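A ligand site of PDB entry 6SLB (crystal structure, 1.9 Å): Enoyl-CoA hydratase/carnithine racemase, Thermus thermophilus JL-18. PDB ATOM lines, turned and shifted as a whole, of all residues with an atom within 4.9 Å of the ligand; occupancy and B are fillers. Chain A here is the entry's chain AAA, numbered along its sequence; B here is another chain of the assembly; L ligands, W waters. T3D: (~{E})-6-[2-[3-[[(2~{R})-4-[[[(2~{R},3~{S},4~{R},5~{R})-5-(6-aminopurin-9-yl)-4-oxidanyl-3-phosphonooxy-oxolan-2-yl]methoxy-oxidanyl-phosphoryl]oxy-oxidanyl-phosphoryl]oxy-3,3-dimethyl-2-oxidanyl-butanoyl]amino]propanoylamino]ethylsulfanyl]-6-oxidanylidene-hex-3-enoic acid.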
ATOM      1  N   LYS A  23      14.325 -11.011  17.897  1.00  0.00           N
ATOM      2  CA  LYS A  23      15.178 -12.188  17.595  1.00  0.00           C
ATOM      3  C   LYS A  23      15.273 -13.061  18.855  1.00  0.00           C
ATOM      4  O   LYS A  23      16.222 -13.833  18.947  1.00  0.00           O
ATOM      5  CB  LYS A  23      16.571 -11.789  17.094  1.00  0.00           C
ATOM      6  CG  LYS A  23      16.747 -11.677  15.582  1.00  0.00           C
ATOM      7  CD  LYS A  23      15.892 -10.566  14.999  1.00  0.00           C
ATOM      8  CE  LYS A  23      16.418  -9.974  13.712  1.00  0.00           C
ATOM      9  NZ  LYS A  23      16.088  -8.536  13.631  1.00  0.00           N
ATOM     10  N   LEU A  24      14.256 -12.986  19.735  1.00  0.00           N
ATOM     11  CA  LEU A  24      14.156 -13.777  20.980  1.00  0.00           C
ATOM     12  C   LEU A  24      15.418 -13.550  21.824  1.00  0.00           C
ATOM     13  O   LEU A  24      15.918 -14.522  22.449  1.00  0.00           O
ATOM     14  CB  LEU A  24      13.970 -15.249  20.640  1.00  0.00           C
ATOM     15  CG  LEU A  24      12.788 -15.591  19.704  1.00  0.00           C
ATOM     16  CD1 LEU A  24      12.624 -17.096  19.589  1.00  0.00           C
ATOM     17  CD2 LEU A  24      11.514 -14.932  20.199  1.00  0.00           C
ATOM     18  N   ALA A  26      18.421 -13.135  20.992  1.00  0.00           N
ATOM     19  CA  ALA A  26      19.580 -13.906  20.473  1.00  0.00           C
ATOM     20  C   ALA A  26      20.849 -13.101  20.726  1.00  0.00           C
ATOM     21  O   ALA A  26      20.815 -11.850  20.571  1.00  0.00           O
ATOM     22  CB  ALA A  26      19.409 -14.269  19.031  1.00  0.00           C
ATOM     23  N   ARG A  58       8.857 -12.389  24.441  1.00  0.00           N
ATOM     24  CA  ARG A  58       8.378 -13.785  24.546  1.00  0.00           C
ATOM     25  C   ARG A  58       9.428 -14.667  25.250  1.00  0.00           C
ATOM     26  O   ARG A  58       9.044 -15.662  25.910  1.00  0.00           O
ATOM     27  CB  ARG A  58       8.239 -14.287  23.096  1.00  0.00           C
ATOM     28  CG  ARG A  58       7.364 -15.495  22.905  1.00  0.00           C
ATOM     29  CD  ARG A  58       6.746 -15.551  21.522  1.00  0.00           C
ATOM     30  NE  ARG A  58       7.672 -15.917  20.446  1.00  0.00           N
ATOM     31  CZ  ARG A  58       8.280 -17.094  20.314  1.00  0.00           C
ATOM     32  NH1 ARG A  58       8.144 -18.034  21.231  1.00  0.00           N
ATOM     33  NH2 ARG A  58       9.074 -17.315  19.274  1.00  0.00           N
ATOM     34  N   ALA A  62      17.245 -17.034  23.188  1.00  0.00           N
ATOM     35  CA  ALA A  62      17.415 -18.203  22.292  1.00  0.00           C
ATOM     36  C   ALA A  62      18.890 -18.536  22.122  1.00  0.00           C
ATOM     37  O   ALA A  62      19.185 -19.423  21.334  1.00  0.00           O
ATOM     38  CB  ALA A  62      16.755 -17.934  20.972  1.00  0.00           C
ATOM     39  N   GLY A  63      19.790 -17.836  22.823  1.00  0.00           N
ATOM     40  CA  GLY A  63      21.216 -18.132  22.776  1.00  0.00           C
ATOM     41  C   GLY A  63      21.869 -17.451  21.582  1.00  0.00           C
ATOM     42  O   GLY A  63      21.301 -16.463  21.088  1.00  0.00           O
ATOM     43  N   GLN A  64      23.008 -17.963  21.144  1.00  0.00           N
ATOM     44  CA  GLN A  64      23.823 -17.336  20.060  1.00  0.00           C
ATOM     45  C   GLN A  64      22.930 -17.067  18.835  1.00  0.00           C
ATOM     46  O   GLN A  64      22.227 -17.983  18.382  1.00  0.00           O
ATOM     47  CB  GLN A  64      25.009 -18.198  19.638  1.00  0.00           C
ATOM     48  CG  GLN A  64      25.721 -17.698  18.369  1.00  0.00           C
ATOM     49  CD  GLN A  64      26.344 -16.340  18.520  1.00  0.00           C
ATOM     50  OE1 GLN A  64      26.938 -16.039  19.534  1.00  0.00           O
ATOM     51  NE2 GLN A  64      26.174 -15.472  17.522  1.00  0.00           N
ATOM     52  N   ASP A  65      23.055 -15.875  18.283  1.00  0.00           N
ATOM     53  CA  ASP A  65      22.393 -15.518  16.997  1.00  0.00           C
ATOM     54  C   ASP A  65      23.075 -16.284  15.868  1.00  0.00           C
ATOM     55  O   ASP A  65      24.234 -15.952  15.502  1.00  0.00           O
ATOM     56  CB  ASP A  65      22.447 -14.024  16.791  1.00  0.00           C
ATOM     57  CG  ASP A  65      21.709 -13.564  15.550  1.00  0.00           C
ATOM     58  OD1 ASP A  65      21.367 -14.398  14.696  1.00  0.00           O
ATOM     59  OD2 ASP A  65      21.429 -12.381  15.523  1.00  0.00           O
ATOM     60  N   LEU A  66      22.369 -17.277  15.347  1.00  0.00           N
ATOM     61  CA  LEU A  66      22.878 -18.199  14.304  1.00  0.00           C
ATOM     62  C   LEU A  66      22.812 -17.531  12.912  1.00  0.00           C
ATOM     63  O   LEU A  66      22.999 -18.273  11.917  1.00  0.00           O
ATOM     64  CB  LEU A  66      22.059 -19.488  14.357  1.00  0.00           C
ATOM     65  CG  LEU A  66      22.212 -20.283  15.646  1.00  0.00           C
ATOM     66  CD1 LEU A  66      21.214 -21.416  15.700  1.00  0.00           C
ATOM     67  CD2 LEU A  66      23.642 -20.801  15.800  1.00  0.00           C
ATOM     68  N   THR A  67      22.619 -16.205  12.866  1.00  0.00           N
ATOM     69  CA  THR A  67      22.891 -15.338  11.664  1.00  0.00           C
ATOM     70  C   THR A  67      24.160 -14.483  11.837  1.00  0.00           C
ATOM     71  O   THR A  67      24.678 -14.028  10.801  1.00  0.00           O
ATOM     72  CB  THR A  67      21.703 -14.421  11.351  1.00  0.00           C
ATOM     73  OG1 THR A  67      20.501 -15.176  11.488  1.00  0.00           O
ATOM     74  CG2 THR A  67      21.779 -13.843   9.954  1.00  0.00           C
ATOM     75  N   TYR A  76      35.592 -20.440  17.004  1.00  0.00           N
ATOM     76  CA  TYR A  76      34.859 -20.386  18.292  1.00  0.00           C
ATOM     77  C   TYR A  76      35.842 -20.271  19.456  1.00  0.00           C
ATOM     78  O   TYR A  76      35.462 -19.649  20.479  1.00  0.00           O
ATOM     79  CB  TYR A  76      33.902 -21.578  18.399  1.00  0.00           C
ATOM     80  CG  TYR A  76      32.761 -21.491  17.423  1.00  0.00           C
ATOM     81  CD1 TYR A  76      32.324 -20.258  16.961  1.00  0.00           C
ATOM     82  CD2 TYR A  76      32.110 -22.620  16.955  1.00  0.00           C
ATOM     83  CE1 TYR A  76      31.273 -20.145  16.065  1.00  0.00           C
ATOM     84  CE2 TYR A  76      31.058 -22.524  16.065  1.00  0.00           C
ATOM     85  CZ  TYR A  76      30.638 -21.282  15.615  1.00  0.00           C
ATOM     86  OH  TYR A  76      29.607 -21.145  14.724  1.00  0.00           O
ATOM     87  N   HIS A  79      36.419 -16.420  19.588  1.00  0.00           N
ATOM     88  CA  HIS A  79      35.146 -15.726  19.918  1.00  0.00           C
ATOM     89  C   HIS A  79      34.769 -15.984  21.376  1.00  0.00           C
ATOM     90  O   HIS A  79      34.341 -15.044  22.046  1.00  0.00           O
ATOM     91  CB  HIS A  79      34.028 -16.156  18.970  1.00  0.00           C
ATOM     92  CG  HIS A  79      32.741 -15.435  19.206  1.00  0.00           C
ATOM     93  ND1 HIS A  79      31.909 -15.722  20.278  1.00  0.00           N
ATOM     94  CD2 HIS A  79      32.130 -14.444  18.514  1.00  0.00           C
ATOM     95  CE1 HIS A  79      30.853 -14.932  20.226  1.00  0.00           C
ATOM     96  NE2 HIS A  79      30.959 -14.148  19.157  1.00  0.00           N
ATOM     97  N   LEU A  80      34.942 -17.218  21.857  1.00  0.00           N
ATOM     98  CA  LEU A  80      34.465 -17.546  23.230  1.00  0.00           C
ATOM     99  C   LEU A  80      35.229 -16.722  24.264  1.00  0.00           C
ATOM    100  O   LEU A  80      34.602 -16.377  25.277  1.00  0.00           O
ATOM    101  CB  LEU A  80      34.547 -19.061  23.458  1.00  0.00           C
ATOM    102  CG  LEU A  80      33.273 -19.810  23.077  1.00  0.00           C
ATOM    103  CD1 LEU A  80      33.358 -21.278  23.506  1.00  0.00           C
ATOM    104  CD2 LEU A  80      32.044 -19.148  23.692  1.00  0.00           C
ATOM    105  N   TYR A  83      32.233 -14.293  25.129  1.00  0.00           N
ATOM    106  CA  TYR A  83      31.328 -15.056  26.047  1.00  0.00           C
ATOM    107  C   TYR A  83      32.069 -15.224  27.380  1.00  0.00           C
ATOM    108  O   TYR A  83      31.385 -15.283  28.429  1.00  0.00           O
ATOM    109  CB  TYR A  83      30.931 -16.449  25.566  1.00  0.00           C
ATOM    110  CG  TYR A  83      29.734 -16.499  24.652  1.00  0.00           C
ATOM    111  CD1 TYR A  83      28.440 -16.513  25.145  1.00  0.00           C
ATOM    112  CD2 TYR A  83      29.896 -16.526  23.270  1.00  0.00           C
ATOM    113  CE1 TYR A  83      27.348 -16.555  24.303  1.00  0.00           C
ATOM    114  CE2 TYR A  83      28.819 -16.591  22.406  1.00  0.00           C
ATOM    115  CZ  TYR A  83      27.536 -16.616  22.926  1.00  0.00           C
ATOM    116  OH  TYR A  83      26.466 -16.652  22.074  1.00  0.00           O
ATOM    117  N   VAL A 104      11.568 -18.808  26.844  1.00  0.00           N
ATOM    118  CA  VAL A 104      12.568 -19.856  26.504  1.00  0.00           C
ATOM    119  C   VAL A 104      13.969 -19.315  26.783  1.00  0.00           C
ATOM    120  O   VAL A 104      14.271 -18.114  26.506  1.00  0.00           O
ATOM    121  CB  VAL A 104      12.428 -20.399  25.078  1.00  0.00           C
ATOM    122  CG1 VAL A 104      12.550 -19.336  24.022  1.00  0.00           C
ATOM    123  CG2 VAL A 104      13.366 -21.563  24.838  1.00  0.00           C
ATOM    124  N   ALA A 106      17.616 -20.987  25.772  1.00  0.00           N
ATOM    125  CA  ALA A 106      18.221 -22.045  24.956  1.00  0.00           C
ATOM    126  C   ALA A 106      19.701 -21.756  24.778  1.00  0.00           C
ATOM    127  O   ALA A 106      20.075 -20.574  24.605  1.00  0.00           O
ATOM    128  CB  ALA A 106      17.529 -22.152  23.624  1.00  0.00           C
ATOM    129  N   GLY A 107      20.525 -22.791  24.732  1.00  0.00           N
ATOM    130  CA  GLY A 107      21.961 -22.625  24.450  1.00  0.00           C
ATOM    131  C   GLY A 107      22.628 -21.689  25.449  1.00  0.00           C
ATOM    132  O   GLY A 107      22.431 -21.859  26.665  1.00  0.00           O
ATOM    133  N   ALA A 108      23.392 -20.704  24.970  1.00  0.00           N
ATOM    134  CA  ALA A 108      24.025 -19.711  25.849  1.00  0.00           C
ATOM    135  C   ALA A 108      22.969 -18.902  26.609  1.00  0.00           C
ATOM    136  O   ALA A 108      23.330 -18.342  27.645  1.00  0.00           O
ATOM    137  CB  ALA A 108      24.981 -18.823  25.063  1.00  0.00           C
ATOM    138  N   THR A 128      16.218 -25.361  27.147  1.00  0.00           N
ATOM    139  CA  THR A 128      16.762 -26.395  26.246  1.00  0.00           C
ATOM    140  C   THR A 128      18.254 -26.115  26.048  1.00  0.00           C
ATOM    141  O   THR A 128      18.646 -24.970  25.724  1.00  0.00           O
ATOM    142  CB  THR A 128      15.908 -26.491  24.981  1.00  0.00           C
ATOM    143  OG1 THR A 128      16.381 -27.678  24.316  1.00  0.00           O
ATOM    144  CG2 THR A 128      15.964 -25.286  24.090  1.00  0.00           C
ATOM    145  N   ALA A 130      20.290 -27.117  23.619  1.00  0.00           N
ATOM    146  CA  ALA A 130      20.323 -26.620  22.224  1.00  0.00           C
ATOM    147  C   ALA A 130      21.642 -26.904  21.490  1.00  0.00           C
ATOM    148  O   ALA A 130      21.569 -27.267  20.289  1.00  0.00           O
ATOM    149  CB  ALA A 130      20.009 -25.139  22.164  1.00  0.00           C
ATOM    150  N   PHE A 131      22.814 -26.763  22.133  1.00  0.00           N
ATOM    151  CA  PHE A 131      24.132 -26.808  21.450  1.00  0.00           C
ATOM    152  C   PHE A 131      24.254 -28.061  20.564  1.00  0.00           C
ATOM    153  O   PHE A 131      24.689 -27.987  19.406  1.00  0.00           O
ATOM    154  CB  PHE A 131      25.275 -26.799  22.464  1.00  0.00           C
ATOM    155  CG  PHE A 131      25.391 -25.539  23.260  1.00  0.00           C
ATOM    156  CD1 PHE A 131      26.020 -24.427  22.740  1.00  0.00           C
ATOM    157  CD2 PHE A 131      24.902 -25.484  24.552  1.00  0.00           C
ATOM    158  CE1 PHE A 131      26.168 -23.285  23.499  1.00  0.00           C
ATOM    159  CE2 PHE A 131      25.021 -24.317  25.301  1.00  0.00           C
ATOM    160  CZ  PHE A 131      25.654 -23.233  24.776  1.00  0.00           C
ATOM    161  N   ILE A 134      23.072 -28.200  16.966  1.00  0.00           N
ATOM    162  CA  ILE A 134      23.894 -27.418  15.973  1.00  0.00           C
ATOM    163  C   ILE A 134      25.256 -28.112  15.832  1.00  0.00           C
ATOM    164  O   ILE A 134      26.170 -27.578  15.163  1.00  0.00           O
ATOM    165  CB  ILE A 134      24.003 -25.959  16.479  1.00  0.00           C
ATOM    166  CG1 ILE A 134      22.634 -25.422  16.902  1.00  0.00           C
ATOM    167  CG2 ILE A 134      24.647 -25.027  15.475  1.00  0.00           C
ATOM    168  CD1 ILE A 134      21.619 -25.523  15.792  1.00  0.00           C
ATOM    169  N   LEU A 136      27.433 -28.629  18.338  1.00  0.00           N
ATOM    170  CA  LEU A 136      28.370 -27.910  19.229  1.00  0.00           C
ATOM    171  C   LEU A 136      28.292 -28.504  20.632  1.00  0.00           C
ATOM    172  O   LEU A 136      27.358 -29.280  20.933  1.00  0.00           O
ATOM    173  CB  LEU A 136      28.002 -26.435  19.278  1.00  0.00           C
ATOM    174  CG  LEU A 136      28.240 -25.676  17.983  1.00  0.00           C
ATOM    175  CD1 LEU A 136      27.914 -24.224  18.178  1.00  0.00           C
ATOM    176  CD2 LEU A 136      29.682 -25.862  17.505  1.00  0.00           C
ATOM    177  N   ASP A 139      28.697 -24.366  26.152  1.00  0.00           N
ATOM    178  CA  ASP A 139      29.688 -23.304  26.392  1.00  0.00           C
ATOM    179  C   ASP A 139      29.077 -22.274  27.325  1.00  0.00           C
ATOM    180  O   ASP A 139      27.992 -22.544  27.924  1.00  0.00           O
ATOM    181  CB  ASP A 139      30.227 -22.761  25.063  1.00  0.00           C
ATOM    182  CG  ASP A 139      29.316 -21.829  24.262  1.00  0.00           C
ATOM    183  OD1 ASP A 139      28.424 -21.150  24.843  1.00  0.00           O
ATOM    184  OD2 ASP A 139      29.580 -21.726  23.041  1.00  0.00           O
ATOM    185  N   GLN B 230      35.022 -26.264  21.678  1.00  0.00           N
ATOM    186  CA  GLN B 230      34.026 -25.590  20.797  1.00  0.00           C
ATOM    187  C   GLN B 230      34.697 -25.166  19.498  1.00  0.00           C
ATOM    188  O   GLN B 230      34.088 -25.324  18.444  1.00  0.00           O
ATOM    189  CB  GLN B 230      33.374 -24.387  21.474  1.00  0.00           C
ATOM    190  CG  GLN B 230      32.131 -23.920  20.730  1.00  0.00           C
ATOM    191  CD  GLN B 230      30.972 -24.857  21.006  1.00  0.00           C
ATOM    192  OE1 GLN B 230      30.977 -26.005  20.552  1.00  0.00           O
ATOM    193  NE2 GLN B 230      29.985 -24.368  21.754  1.00  0.00           N
ATOM    194  N   PHE B 246      19.173 -25.423  10.864  1.00  0.00           N
ATOM    195  CA  PHE B 246      18.437 -24.465  11.698  1.00  0.00           C
ATOM    196  C   PHE B 246      17.921 -23.318  10.831  1.00  0.00           C
ATOM    197  O   PHE B 246      16.733 -23.013  10.917  1.00  0.00           O
ATOM    198  CB  PHE B 246      19.260 -23.955  12.893  1.00  0.00           C
ATOM    199  CG  PHE B 246      18.477 -22.901  13.622  1.00  0.00           C
ATOM    200  CD1 PHE B 246      17.518 -23.261  14.558  1.00  0.00           C
ATOM    201  CD2 PHE B 246      18.611 -21.568  13.288  1.00  0.00           C
ATOM    202  CE1 PHE B 246      16.744 -22.293  15.199  1.00  0.00           C
ATOM    203  CE2 PHE B 246      17.850 -20.599  13.936  1.00  0.00           C
ATOM    204  CZ  PHE B 246      16.923 -20.958  14.901  1.00  0.00           C
ATOM    205  N   LYS B 249      15.067 -24.491   8.806  1.00  0.00           N
ATOM    206  CA  LYS B 249      14.091 -25.134   9.716  1.00  0.00           C
ATOM    207  C   LYS B 249      13.773 -26.533   9.183  1.00  0.00           C
ATOM    208  O   LYS B 249      12.586 -26.818   8.961  1.00  0.00           O
ATOM    209  CB  LYS B 249      12.852 -24.245   9.871  1.00  0.00           C
ATOM    210  CG  LYS B 249      13.111 -22.870  10.483  1.00  0.00           C
ATOM    211  CD  LYS B 249      13.579 -22.983  11.926  1.00  0.00           C
ATOM    212  CE  LYS B 249      13.881 -21.637  12.542  1.00  0.00           C
ATOM    213  NZ  LYS B 249      14.900 -20.902  11.785  1.00  0.00           N
HETATM  214  O1  T3D L   1      28.526 -19.940  17.752  1.00  0.00           O
HETATM  215  C1  T3D L   1      29.431 -19.606  18.559  1.00  0.00           C
HETATM  216  O2  T3D L   1      30.019 -18.485  18.651  1.00  0.00           O
HETATM  217  C2  T3D L   1      29.824 -20.643  19.552  1.00  0.00           C
HETATM  218  C3  T3D L   1      28.826 -20.323  20.648  1.00  0.00           C
HETATM  219  C4  T3D L   1      27.392 -20.874  20.571  1.00  0.00           C
HETATM  220  C5  T3D L   1      26.499 -20.527  21.708  1.00  0.00           C
HETATM  221  C6  T3D L   1      25.026 -21.034  21.493  1.00  0.00           C
HETATM  222  O3  T3D L   1      24.157 -20.447  22.133  1.00  0.00           O
HETATM  223  S1  T3D L   1      24.656 -22.348  20.205  1.00  0.00           S
HETATM  224  C7  T3D L   1      22.883 -22.650  20.582  1.00  0.00           C
HETATM  225  C8  T3D L   1      22.246 -21.518  19.843  1.00  0.00           C
HETATM  226  N1  T3D L   1      20.780 -21.570  20.057  1.00  0.00           N
HETATM  227  C9  T3D L   1      19.977 -22.441  19.445  1.00  0.00           C
HETATM  228  O4  T3D L   1      20.407 -23.444  18.852  1.00  0.00           O
HETATM  229  C10 T3D L   1      18.461 -22.223  19.645  1.00  0.00           C
HETATM  230  C11 T3D L   1      17.875 -22.292  18.252  1.00  0.00           C
HETATM  231  N2  T3D L   1      16.403 -22.013  18.352  1.00  0.00           N
HETATM  232  C12 T3D L   1      15.494 -22.880  18.795  1.00  0.00           C
HETATM  233  O5  T3D L   1      15.747 -24.072  19.015  1.00  0.00           O
HETATM  234  C13 T3D L   1      14.063 -22.342  18.868  1.00  0.00           C
HETATM  235  O6  T3D L   1      13.942 -21.159  18.004  1.00  0.00           O
HETATM  236  C14 T3D L   1      13.678 -21.920  20.303  1.00  0.00           C
HETATM  237  C15 T3D L   1      14.752 -20.934  20.883  1.00  0.00           C
HETATM  238  C16 T3D L   1      13.568 -23.111  21.273  1.00  0.00           C
HETATM  239  C17 T3D L   1      12.345 -21.168  20.300  1.00  0.00           C
HETATM  240  O7  T3D L   1      11.311 -21.880  19.521  1.00  0.00           O
HETATM  241  P1  T3D L   1      10.074 -20.999  19.101  1.00  0.00           P
HETATM  242  O8  T3D L   1       9.036 -21.916  18.548  1.00  0.00           O
HETATM  243  O9  T3D L   1       9.751 -20.108  20.238  1.00  0.00           O
HETATM  244  O10 T3D L   1      10.576 -20.023  17.938  1.00  0.00           O
HETATM  245  P2  T3D L   1      11.047 -20.468  16.427  1.00  0.00           P
HETATM  246  O11 T3D L   1       9.790 -20.631  15.650  1.00  0.00           O
HETATM  247  O12 T3D L   1      12.000 -21.572  16.422  1.00  0.00           O
HETATM  248  O13 T3D L   1      11.826 -19.140  15.965  1.00  0.00           O
HETATM  249  C18 T3D L   1      11.138 -17.930  15.804  1.00  0.00           C
HETATM  250  C19 T3D L   1      12.134 -16.991  15.112  1.00  0.00           C
HETATM  251  O14 T3D L   1      13.387 -16.675  15.928  1.00  0.00           O
HETATM  252  C20 T3D L   1      12.654 -17.596  13.785  1.00  0.00           C
HETATM  253  O15 T3D L   1      12.897 -16.522  12.845  1.00  0.00           O
HETATM  254  P3  T3D L   1      11.867 -16.147  11.655  1.00  0.00           P
HETATM  255  O16 T3D L   1      10.760 -15.563  12.398  1.00  0.00           O
HETATM  256  O17 T3D L   1      12.585 -15.232  10.839  1.00  0.00           O
HETATM  257  O18 T3D L   1      11.621 -17.445  11.036  1.00  0.00           O
HETATM  258  C21 T3D L   1      14.020 -18.168  14.287  1.00  0.00           C
HETATM  259  O19 T3D L   1      15.025 -18.440  13.302  1.00  0.00           O
HETATM  260  C22 T3D L   1      14.514 -17.089  15.195  1.00  0.00           C
HETATM  261  N3  T3D L   1      15.448 -17.658  16.210  1.00  0.00           N
HETATM  262  C23 T3D L   1      15.252 -18.522  17.220  1.00  0.00           C
HETATM  263  N4  T3D L   1      16.427 -18.825  17.771  1.00  0.00           N
HETATM  264  C24 T3D L   1      17.371 -18.112  17.107  1.00  0.00           C
HETATM  265  C25 T3D L   1      16.759 -17.453  16.128  1.00  0.00           C
HETATM  266  N5  T3D L   1      17.439 -16.742  15.225  1.00  0.00           N
HETATM  267  C26 T3D L   1      18.802 -16.565  15.199  1.00  0.00           C
HETATM  268  N6  T3D L   1      19.404 -17.313  16.266  1.00  0.00           N
HETATM  269  C27 T3D L   1      18.707 -17.998  17.166  1.00  0.00           C
HETATM  270  N7  T3D L   1      19.372 -18.626  18.148  1.00  0.00           N
HETATM  271  O   HOH W   1      17.231 -26.003  20.345  1.00  0.00           O
HETATM  272  O   HOH W   2      13.054 -19.122  10.041  1.00  0.00           O
HETATM  273  O   HOH W   3       9.171 -21.380  22.544  1.00  0.00           O
HETATM  274  O   HOH W   4      12.445 -23.834  15.434  1.00  0.00           O
HETATM  275  O   HOH W   5      19.570 -25.878  18.533  1.00  0.00           O
HETATM  276  O   HOH W   6       9.196 -15.456  17.177  1.00  0.00           O
HETATM  277  O   HOH W   7      15.289 -26.089  16.895  1.00  0.00           O
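Water W2 lies within hydrogen-bond range of O18 of the ligand (2.4 Å) and NZ of Lys 249 of chain B (3.1 Å).
Water W5 lies within hydrogen-bond range of an oxygen (O4) of the ligand (2.6 Å) and the backbone carbonyl oxygen (O) of Ala 130 (3.0 Å).
Leu 24 touches the ligand (CD1 to O14, 3.8 Å).
CA of Gly 63 touches O3 of the ligand, at 3.8 Å.
Asp 65 touches the ligand.
ND1 of His 79 touches O2 of the ligand (3.7 Å).
OH of Tyr 83 touches C5 of the ligand, at 3.9 Å.
Val 104 touches the ligand (CG2 to C16, 3.9 Å).
C of Gly 107 touches O3 of the ligand (3.9 Å).
Ala 130 touches the ligand.
Phe 131 touches the ligand.
CG1 of Ile 134 touches O4 of the ligand, 3.6 Å away.
OD2 of Asp 139 touches C3 of the ligand, at 2.9 Å.
Phe 246 of chain B touches the ligand (CE1 to N2, 3.2 Å).
Hydrophobic or aromatic side chains within 4 Å of the ligand: Leu 24, Ala 62, Leu 66, Tyr 76, His 79, Val 104, Ala 108, Ala 130, Phe 131, Ile 134 and Phe 246 of chain B.
Of the 27 residues printed, 19 come within 4 Å of the ligand.
The nearest printed residue that does not touch the ligand is Ala 106 (4.1 Å).
The guanidinium group (NH1) of Arg 58 lies within salt-bridge range of an oxygen (O9) of the ligand (2.8 Å).
The side-chain amino group of Lys 249 of chain B sits at hydrogen-bond distance from an oxygen (O19) of the ligand (2.9 Å).
N of Gln 64 lies within hydrogen-bond range of O3 of the ligand (2.9 Å).
A nitrogen (N7) of the ligand is in hydrogen-bond range of the backbone carbonyl oxygen (O) of Gln 64, at 2.9 Å.
The backbone NH of Ala 108 is in hydrogen-bond range of an oxygen (O3) of the ligand.
The backbone carbonyl oxygen of Ala 62 sits at hydrogen-bond distance from a nitrogen (N1) of the ligand (3.0 Å).
The backbone NH (N) of Leu 66 is in hydrogen-bond range of a nitrogen (N6) of the ligand.
The side-chain hydroxyl (OH) of Tyr 76 lies close to an oxygen (O1) of the ligand.
NE2 of Gln 230 of chain B is in hydrogen-bond range of OD2 of Asp 139, 3.0 Å away.
The backbone carbonyl oxygen (O) of Phe 246 of chain B sits at hydrogen-bond distance from the side-chain amino group (NZ) of Lys 249 of chain B (2.9 Å).
OE1 of Gln 64 lies within hydrogen-bond range of OH of Tyr 83 (2.7 Å).
The backbone carbonyl oxygen (O) of Leu 24 is in hydrogen-bond range of the backbone NH (N) of Ala 62, 2.9 Å away.
The backbone NH (N) of Leu 136 is in hydrogen-bond range of the backbone carbonyl oxygen (O) of Phe 131 (3.0 Å).
The backbone NH of Thr 67 is in hydrogen-bond range of the side-chain carboxylate of Asp 65 (2.9 Å).
O of Ala 106 sits close to N of Gly 63, at 3.3 Å.
The backbone carbonyl oxygen (O) of Thr 128 is in hydrogen-bond range of the backbone NH (N) of Gly 107 (3.0 Å).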
